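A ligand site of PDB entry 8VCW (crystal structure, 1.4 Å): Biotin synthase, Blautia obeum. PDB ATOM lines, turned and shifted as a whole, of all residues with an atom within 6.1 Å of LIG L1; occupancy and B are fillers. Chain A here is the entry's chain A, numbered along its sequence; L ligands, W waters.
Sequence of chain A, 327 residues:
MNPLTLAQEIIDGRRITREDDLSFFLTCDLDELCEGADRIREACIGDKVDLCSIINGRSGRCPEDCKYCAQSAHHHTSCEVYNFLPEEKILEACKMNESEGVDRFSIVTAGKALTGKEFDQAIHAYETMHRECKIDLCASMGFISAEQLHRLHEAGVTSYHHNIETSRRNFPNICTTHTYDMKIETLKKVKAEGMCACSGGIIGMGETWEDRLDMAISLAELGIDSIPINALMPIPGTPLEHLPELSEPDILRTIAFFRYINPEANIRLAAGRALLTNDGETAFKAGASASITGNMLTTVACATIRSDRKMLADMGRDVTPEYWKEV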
ATOM      1  N   ILE A  54      -6.272   2.670   0.400  1.00  0.00           N
ATOM      2  CA  ILE A  54      -5.387   1.661   0.958  1.00  0.00           C
ATOM      3  C   ILE A  54      -4.418   2.273   1.949  1.00  0.00           C
ATOM      4  O   ILE A  54      -4.056   3.455   1.838  1.00  0.00           O
ATOM      5  CB  ILE A  54      -4.638   0.886  -0.161  1.00  0.00           C
ATOM      6  CG1 ILE A  54      -3.611   1.754  -0.883  1.00  0.00           C
ATOM      7  CG2 ILE A  54      -5.623   0.258  -1.158  1.00  0.00           C
ATOM      8  CD1 ILE A  54      -2.900   1.006  -2.027  1.00  0.00           C
ATOM      9  N   ALA A  70       8.352  -2.917  -5.566  1.00  0.00           N
ATOM     10  CA  ALA A  70       9.277  -2.164  -4.745  1.00  0.00           C
ATOM     11  C   ALA A  70       9.555  -2.852  -3.405  1.00  0.00           C
ATOM     12  O   ALA A  70      10.591  -2.528  -2.784  1.00  0.00           O
ATOM     13  CB  ALA A  70       8.707  -0.775  -4.478  1.00  0.00           C
ATOM     14  N   GLN A  71       8.649  -3.727  -2.931  1.00  0.00           N
ATOM     15  CA  GLN A  71       8.767  -4.242  -1.572  1.00  0.00           C
ATOM     16  C   GLN A  71       9.455  -5.595  -1.504  1.00  0.00           C
ATOM     17  O   GLN A  71       9.568  -6.170  -0.398  1.00  0.00           O
ATOM     18  CB  GLN A  71       7.429  -4.254  -0.868  1.00  0.00           C
ATOM     19  CG  GLN A  71       6.724  -2.917  -0.955  1.00  0.00           C
ATOM     20  CD  GLN A  71       5.565  -2.800  -0.067  1.00  0.00           C
ATOM     21  OE1 GLN A  71       5.646  -2.956   1.144  1.00  0.00           O
ATOM     22  NE2 GLN A  71       4.407  -2.548  -0.648  1.00  0.00           N
ATOM     23  N   VAL A 108      -3.073  -3.365   3.316  1.00  0.00           N
ATOM     24  CA  VAL A 108      -2.284  -4.114   2.334  1.00  0.00           C
ATOM     25  C   VAL A 108      -0.915  -4.417   2.922  1.00  0.00           C
ATOM     26  O   VAL A 108      -0.221  -3.490   3.345  1.00  0.00           O
ATOM     27  CB  VAL A 108      -2.087  -3.261   1.082  1.00  0.00           C
ATOM     28  CG1 VAL A 108      -1.298  -4.048   0.037  1.00  0.00           C
ATOM     29  CG2 VAL A 108      -3.428  -2.836   0.531  1.00  0.00           C
ATOM     30  N   SER A 140      -5.692  -7.035   1.753  1.00  0.00           N
ATOM     31  CA  SER A 140      -4.785  -7.608   0.747  1.00  0.00           C
ATOM     32  C   SER A 140      -3.565  -8.130   1.484  1.00  0.00           C
ATOM     33  O   SER A 140      -2.672  -7.352   1.854  1.00  0.00           O
ATOM     34  CB  SER A 140      -4.402  -6.523  -0.239  1.00  0.00           C
ATOM     35  OG  SER A 140      -3.635  -7.103  -1.294  1.00  0.00           O
ATOM     36  N   HIS A 161      -8.498  -8.839  -1.631  1.00  0.00           N
ATOM     37  CA  HIS A 161      -7.768  -8.500  -2.841  1.00  0.00           C
ATOM     38  C   HIS A 161      -6.652  -9.508  -3.068  1.00  0.00           C
ATOM     39  O   HIS A 161      -5.823  -9.774  -2.175  1.00  0.00           O
ATOM     40  CB  HIS A 161      -7.133  -7.132  -2.616  1.00  0.00           C
ATOM     41  CG  HIS A 161      -6.308  -6.667  -3.768  1.00  0.00           C
ATOM     42  ND1 HIS A 161      -4.922  -6.678  -3.758  1.00  0.00           N
ATOM     43  CD2 HIS A 161      -6.688  -6.176  -4.971  1.00  0.00           C
ATOM     44  CE1 HIS A 161      -4.503  -6.207  -4.938  1.00  0.00           C
ATOM     45  NE2 HIS A 161      -5.540  -5.867  -5.662  1.00  0.00           N
ATOM     46  N   ASN A 163      -4.413 -10.138  -6.654  1.00  0.00           N
ATOM     47  CA  ASN A 163      -4.272  -9.978  -8.096  1.00  0.00           C
ATOM     48  C   ASN A 163      -3.627 -11.197  -8.730  1.00  0.00           C
ATOM     49  O   ASN A 163      -2.725 -11.830  -8.170  1.00  0.00           O
ATOM     50  CB  ASN A 163      -3.351  -8.775  -8.352  1.00  0.00           C
ATOM     51  CG  ASN A 163      -4.089  -7.464  -8.243  1.00  0.00           C
ATOM     52  OD1 ASN A 163      -5.309  -7.408  -8.279  1.00  0.00           O
ATOM     53  ND2 ASN A 163      -3.345  -6.396  -8.143  1.00  0.00           N
ATOM     54  N   GLY A 200      -7.094  -8.272 -10.230  1.00  0.00           N
ATOM     55  CA  GLY A 200      -6.700  -7.810 -11.543  1.00  0.00           C
ATOM     56  C   GLY A 200      -5.231  -8.015 -11.707  1.00  0.00           C
ATOM     57  O   GLY A 200      -4.701  -9.093 -11.423  1.00  0.00           O
ATOM     58  N   GLY A 201      -4.531  -7.004 -12.206  1.00  0.00           N
ATOM     59  CA  GLY A 201      -3.109  -7.201 -12.394  1.00  0.00           C
ATOM     60  C   GLY A 201      -2.492  -5.936 -12.940  1.00  0.00           C
ATOM     61  O   GLY A 201      -3.012  -4.837 -12.728  1.00  0.00           O
ATOM     62  N   PRO A 228      -9.018  -4.470 -10.514  1.00  0.00           N
ATOM     63  CA  PRO A 228      -8.053  -3.353 -10.624  1.00  0.00           C
ATOM     64  C   PRO A 228      -7.110  -3.559 -11.793  1.00  0.00           C
ATOM     65  O   PRO A 228      -6.380  -4.576 -11.844  1.00  0.00           O
ATOM     66  CB  PRO A 228      -7.291  -3.380  -9.288  1.00  0.00           C
ATOM     67  CG  PRO A 228      -7.668  -4.678  -8.604  1.00  0.00           C
ATOM     68  CD  PRO A 228      -8.770  -5.368  -9.373  1.00  0.00           C
ATOM     69  N   ILE A 229      -7.079  -2.594 -12.703  1.00  0.00           N
ATOM     70  CA  ILE A 229      -6.166  -2.586 -13.838  1.00  0.00           C
ATOM     71  C   ILE A 229      -5.077  -1.580 -13.495  1.00  0.00           C
ATOM     72  O   ILE A 229      -5.271  -0.375 -13.570  1.00  0.00           O
ATOM     73  CB  ILE A 229      -6.892  -2.265 -15.149  1.00  0.00           C
ATOM     74  CG1 ILE A 229      -7.979  -3.353 -15.390  1.00  0.00           C
ATOM     75  CG2 ILE A 229      -5.879  -2.266 -16.245  1.00  0.00           C
ATOM     76  CD1 ILE A 229      -8.757  -3.004 -16.647  1.00  0.00           C
ATOM     77  N   ASN A 230      -3.945  -2.095 -13.062  1.00  0.00           N
ATOM     78  CA  ASN A 230      -2.793  -1.252 -12.750  1.00  0.00           C
ATOM     79  C   ASN A 230      -1.955  -1.096 -13.988  1.00  0.00           C
ATOM     80  O   ASN A 230      -1.668  -2.088 -14.640  1.00  0.00           O
ATOM     81  CB  ASN A 230      -1.882  -1.929 -11.706  1.00  0.00           C
ATOM     82  CG  ASN A 230      -2.567  -2.114 -10.369  1.00  0.00           C
ATOM     83  OD1 ASN A 230      -2.513  -1.226  -9.487  1.00  0.00           O
ATOM     84  ND2 ASN A 230      -3.235  -3.208 -10.206  1.00  0.00           N
ATOM     85  N   MET A 233       4.035   1.037 -12.835  1.00  0.00           N
ATOM     86  CA  MET A 233       4.856   2.151 -12.382  1.00  0.00           C
ATOM     87  C   MET A 233       6.276   1.594 -12.255  1.00  0.00           C
ATOM     88  O   MET A 233       6.573   0.891 -11.301  1.00  0.00           O
ATOM     89  CB  MET A 233       4.342   2.639 -11.024  1.00  0.00           C
ATOM     90  CG  MET A 233       2.940   3.228 -11.203  1.00  0.00           C
ATOM     91  SD  MET A 233       2.263   3.882  -9.640  1.00  0.00           S
ATOM     92  CE  MET A 233       3.076   5.478  -9.561  1.00  0.00           C
ATOM     93  N   ILE A 235       9.693   0.805 -11.025  1.00  0.00           N
ATOM     94  CA  ILE A 235      10.298   1.197  -9.754  1.00  0.00           C
ATOM     95  C   ILE A 235      11.821   1.156  -9.893  1.00  0.00           C
ATOM     96  O   ILE A 235      12.366   0.094 -10.194  1.00  0.00           O
ATOM     97  CB  ILE A 235       9.884   0.269  -8.620  1.00  0.00           C
ATOM     98  CG1 ILE A 235       8.345   0.227  -8.498  1.00  0.00           C
ATOM     99  CG2 ILE A 235      10.563   0.683  -7.329  1.00  0.00           C
ATOM    100  CD1 ILE A 235       7.712   1.618  -8.161  1.00  0.00           C
ATOM    101  N   ALA A 270      -6.282   1.942 -10.904  1.00  0.00           N
ATOM    102  CA  ALA A 270      -5.443   1.579  -9.767  1.00  0.00           C
ATOM    103  C   ALA A 270      -4.106   2.275 -10.005  1.00  0.00           C
ATOM    104  O   ALA A 270      -4.105   3.487 -10.278  1.00  0.00           O
ATOM    105  CB  ALA A 270      -5.350   0.068  -9.682  1.00  0.00           C
ATOM    106  N   ALA A 271      -2.979   1.583  -9.922  1.00  0.00           N
ATOM    107  CA  ALA A 271      -1.716   2.274 -10.095  1.00  0.00           C
ATOM    108  C   ALA A 271      -1.570   2.797 -11.511  1.00  0.00           C
ATOM    109  O   ALA A 271      -2.131   2.266 -12.469  1.00  0.00           O
ATOM    110  CB  ALA A 271      -0.562   1.318  -9.844  1.00  0.00           C
ATOM    111  N   ILE A 292      -9.123   3.215  -7.229  1.00  0.00           N
ATOM    112  CA  ILE A 292      -8.389   3.523  -5.998  1.00  0.00           C
ATOM    113  C   ILE A 292      -8.064   5.013  -6.028  1.00  0.00           C
ATOM    114  O   ILE A 292      -7.737   5.601  -7.088  1.00  0.00           O
ATOM    115  CB  ILE A 292      -7.071   2.742  -5.947  1.00  0.00           C
ATOM    116  CG1 ILE A 292      -7.290   1.252  -6.299  1.00  0.00           C
ATOM    117  CG2 ILE A 292      -6.460   2.898  -4.537  1.00  0.00           C
ATOM    118  CD1 ILE A 292      -6.002   0.401  -6.043  1.00  0.00           C
ATOM    119  N   MET A 296      -0.728   5.477  -2.656  1.00  0.00           N
ATOM    120  CA  MET A 296      -0.577   4.066  -2.949  1.00  0.00           C
ATOM    121  C   MET A 296       0.380   3.501  -1.891  1.00  0.00           C
ATOM    122  O   MET A 296       0.399   3.972  -0.760  1.00  0.00           O
ATOM    123  CB  MET A 296      -0.067   3.806  -4.391  1.00  0.00           C
ATOM    124  CG  MET A 296      -1.082   4.140  -5.515  1.00  0.00           C
ATOM    125  SD  MET A 296      -2.565   3.194  -5.519  1.00  0.00           S
ATOM    126  CE  MET A 296      -3.707   4.504  -5.972  1.00  0.00           C
ATOM    127  N   LEU A 297       1.170   2.490  -2.241  1.00  0.00           N
ATOM    128  CA  LEU A 297       1.910   1.734  -1.226  1.00  0.00           C
ATOM    129  C   LEU A 297       3.278   2.330  -0.980  1.00  0.00           C
ATOM    130  O   LEU A 297       3.721   2.425   0.187  1.00  0.00           O
ATOM    131  CB  LEU A 297       2.047   0.266  -1.636  1.00  0.00           C
ATOM    132  CG  LEU A 297       0.722  -0.459  -1.705  1.00  0.00           C
ATOM    133  CD1 LEU A 297       0.982  -1.838  -2.245  1.00  0.00           C
ATOM    134  CD2 LEU A 297       0.033  -0.520  -0.343  1.00  0.00           C
ATOM    135  N   THR A 298       4.014   2.601  -2.040  1.00  0.00           N
ATOM    136  CA  THR A 298       5.342   3.206  -1.933  1.00  0.00           C
ATOM    137  C   THR A 298       5.461   4.416  -2.851  1.00  0.00           C
ATOM    138  O   THR A 298       6.562   5.010  -2.947  1.00  0.00           O
ATOM    139  CB  THR A 298       6.471   2.196  -2.268  1.00  0.00           C
ATOM    140  OG1 THR A 298       6.482   1.933  -3.685  1.00  0.00           O
ATOM    141  CG2 THR A 298       6.351   0.890  -1.468  1.00  0.00           C
ATOM    142  N   THR A 299       4.386   4.786  -3.550  1.00  0.00           N
ATOM    143  CA  THR A 299       4.355   5.910  -4.479  1.00  0.00           C
ATOM    144  C   THR A 299       3.237   6.835  -4.036  1.00  0.00           C
ATOM    145  O   THR A 299       2.280   6.424  -3.398  1.00  0.00           O
ATOM    146  CB  THR A 299       4.151   5.389  -5.924  1.00  0.00           C
ATOM    147  OG1 THR A 299       2.956   4.573  -5.990  1.00  0.00           O
ATOM    148  CG2 THR A 299       5.299   4.495  -6.371  1.00  0.00           C
ATOM    149  N   VAL A 300       3.297   8.127  -4.495  1.00  0.00           N
ATOM    150  CA  VAL A 300       2.284   9.081  -4.063  1.00  0.00           C
ATOM    151  C   VAL A 300       1.118   9.108  -5.043  1.00  0.00           C
ATOM    152  O   VAL A 300       1.210   8.608  -6.185  1.00  0.00           O
ATOM    153  CB  VAL A 300       2.747  10.512  -3.743  1.00  0.00           C
ATOM    154  CG1 VAL A 300       3.816  10.484  -2.625  1.00  0.00           C
ATOM    155  CG2 VAL A 300       3.164  11.286  -5.010  1.00  0.00           C
HETATM  156  C1  LIG L   1      -4.121  -2.953  -6.669  1.00  0.00           C
HETATM  157  O1  LIG L   1      -4.529  -3.720  -7.496  1.00  0.00           O
HETATM  158  N1  LIG L   1      -2.970  -2.129  -6.770  1.00  0.00           N
HETATM  159  C2  LIG L   1      -2.877  -1.291  -5.577  1.00  0.00           C
HETATM  160  C3  LIG L   1      -3.817  -1.824  -4.561  1.00  0.00           C
HETATM  161  N2  LIG L   1      -4.630  -2.734  -5.341  1.00  0.00           N
HETATM  162  C4  LIG L   1      -3.065  -2.753  -3.571  1.00  0.00           C
HETATM  163  C5  LIG L   1      -1.423  -1.017  -5.162  1.00  0.00           C
HETATM  164  C6  LIG L   1      -0.650  -0.283  -6.266  1.00  0.00           C
HETATM  165  C7  LIG L   1       0.845  -0.185  -5.893  1.00  0.00           C
HETATM  166  C8  LIG L   1       1.584   0.727  -6.898  1.00  0.00           C
HETATM  167  C9  LIG L   1       3.117   0.686  -6.676  1.00  0.00           C
HETATM  168  C10 LIG L   1       3.582   1.151  -5.264  1.00  0.00           C
HETATM  169  O2  LIG L   1       4.583   0.525  -4.764  1.00  0.00           O
HETATM  170  O3  LIG L   1       3.014   2.102  -4.660  1.00  0.00           O
HETATM  171  N1  LG2 L   2       1.868  -9.325  -0.853  1.00  0.00           N
HETATM  172  C1  LG2 L   2       0.437  -9.435  -1.161  1.00  0.00           C
HETATM  173  C2  LG2 L   2       0.208  -9.877  -2.591  1.00  0.00           C
HETATM  174  O1  LG2 L   2       1.166  -9.833  -3.419  1.00  0.00           O
HETATM  175  O2  LG2 L   2      -0.930 -10.264  -2.909  1.00  0.00           O
HETATM  176  C3  LG2 L   2      -0.259  -8.094  -0.837  1.00  0.00           C
HETATM  177  C4  LG2 L   2       0.262  -6.845  -1.579  1.00  0.00           C
HETATM  178  S1  LG2 L   2       0.010  -6.807  -3.367  1.00  0.00           S
HETATM  179  C5  LG2 L   2      -1.762  -6.511  -3.386  1.00  0.00           C
HETATM  180  C6  LG2 L   2       0.340  -5.144  -4.013  1.00  0.00           C
HETATM  181  C7  LG2 L   2      -0.227  -4.960  -5.452  1.00  0.00           C
HETATM  182  O3  LG2 L   2       0.375  -3.798  -5.993  1.00  0.00           O
HETATM  183  C8  LG2 L   2       0.228  -6.079  -6.346  1.00  0.00           C
HETATM  184  O4  LG2 L   2      -0.836  -7.049  -6.344  1.00  0.00           O
HETATM  185  C9  LG2 L   2       0.478  -5.433  -7.684  1.00  0.00           C
HETATM  186  O5  LG2 L   2      -0.551  -5.695  -8.614  1.00  0.00           O
HETATM  187  C10 LG2 L   2       0.464  -3.909  -7.401  1.00  0.00           C
HETATM  188  N2  LG2 L   2       1.801  -3.304  -7.693  1.00  0.00           N
HETATM  189  C11 LG2 L   2       2.932  -3.523  -6.975  1.00  0.00           C
HETATM  190  N3  LG2 L   2       3.933  -2.900  -7.602  1.00  0.00           N
HETATM  191  C12 LG2 L   2       3.447  -2.221  -8.699  1.00  0.00           C
HETATM  192  C13 LG2 L   2       4.000  -1.420  -9.653  1.00  0.00           C
HETATM  193  N4  LG2 L   2       5.330  -1.089  -9.682  1.00  0.00           N
HETATM  194  N5  LG2 L   2       3.241  -0.896 -10.653  1.00  0.00           N
HETATM  195  C14 LG2 L   2       1.910  -1.219 -10.682  1.00  0.00           C
HETATM  196  N6  LG2 L   2       1.321  -2.006  -9.760  1.00  0.00           N
HETATM  197  C15 LG2 L   2       2.089  -2.512  -8.761  1.00  0.00           C
HETATM  198  S1  LG3 L   3      -9.765  -4.841  -2.360  1.00  0.00           S
HETATM  199 FE1  LG3 L   3     -10.127  -3.919  -4.329  1.00  0.00          FE
HETATM  200 FE2  LG3 L   3      -8.269  -3.146  -2.562  1.00  0.00          FE
HETATM  201 FE3  LG3 L   3     -10.902  -3.001  -1.860  1.00  0.00          FE
HETATM  202  S2  LG3 L   3     -11.776  -2.508  -3.849  1.00  0.00           S
HETATM  203 FE4  LG3 L   3      -9.874  -1.283  -3.741  1.00  0.00          FE
HETATM  204  S3  LG3 L   3      -8.395  -2.559  -4.782  1.00  0.00           S
HETATM  205  S4  LG3 L   3      -9.304  -1.417  -1.600  1.00  0.00           S
HETATM  206  S5  LG3 L   3      -6.272  -3.653  -1.779  1.00  0.00           S
HETATM  207  O   HOH W   1       5.944  -1.498  -6.215  1.00  0.00           O
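The side-chain amide nitrogen (ND2) of Asn 163 is in hydrogen-bond range of an oxygen (O1) of LIG L1, at 3.0 Å. N of Thr 299 sits at hydrogen-bond distance from O3 of LIG L1 (3.2 Å). An oxygen (O5) of LG2 L2 lies within hydrogen-bond range of the side-chain amide nitrogen (ND2) of Asn 163 (2.9 Å). OD1 of Asn 230 lies within hydrogen-bond range of N1 of LIG L1, at 2.9 Å. A ring nitrogen (NE2) of His 161 sits at hydrogen-bond distance from an oxygen (O1) of LIG L1. The backbone NH (N) of Met 233 is in hydrogen-bond range of a nitrogen (N5) of LG2 L2 (3.0 Å). The side-chain hydroxyl of Thr 298 lies within hydrogen-bond range of an oxygen (O2) of LIG L1, at 2.6 Å. The side-chain hydroxyl of Thr 299 lies within hydrogen-bond range of an oxygen (O3) of LIG L1 (2.8 Å). The backbone carbonyl oxygen of Met 233 lies within hydrogen-bond range of a nitrogen (N4) of LG2 L2, at 2.8 Å. N of Leu 297 lies within hydrogen-bond range of O3 of LIG L1, at 3.1 Å. N of Thr 298 is in hydrogen-bond range of O3 of LIG L1, 2.8 Å away.
The side-chain hydroxyl (OG1) of Thr 299 sits close to the side-chain sulfur (SD) of Met 233 (3.8 Å). OD1 of Asn 230 is in hydrogen-bond range of N of Ala 271, at 2.9 Å. NE2 of His 161 sits at hydrogen-bond distance from OD1 of Asn 163, at 3.0 Å. N of Asn 230 lies within hydrogen-bond range of O of Gly 201 (2.9 Å). O of Pro 228 sits at hydrogen-bond distance from N of Gly 201 (3.1 Å). The side-chain amide oxygen (OD1) of Asn 163 lies within hydrogen-bond range of the backbone NH (N) of Gly 200, 2.8 Å away. A ring nitrogen (ND1) of His 161 sits at hydrogen-bond distance from the side-chain hydroxyl of Ser 140, at 2.8 Å.
Merely in contact with LIG L1: Ile 54, Pro 228, Ala 271, Ile 292 and Met 296. Within 4 Å of LIG L1: Ile 54, His 161, Asn 163, Pro 228, Asn 230, Ala 271, Ile 292, Met 296, Leu 297, Thr 298 and Thr 299.
Water W1 lies within hydrogen-bond range of N3 of LG2 L2 (2.8 Å), O2 of LIG L1 (2.8 Å) and N of Ala 70 (2.9 Å).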
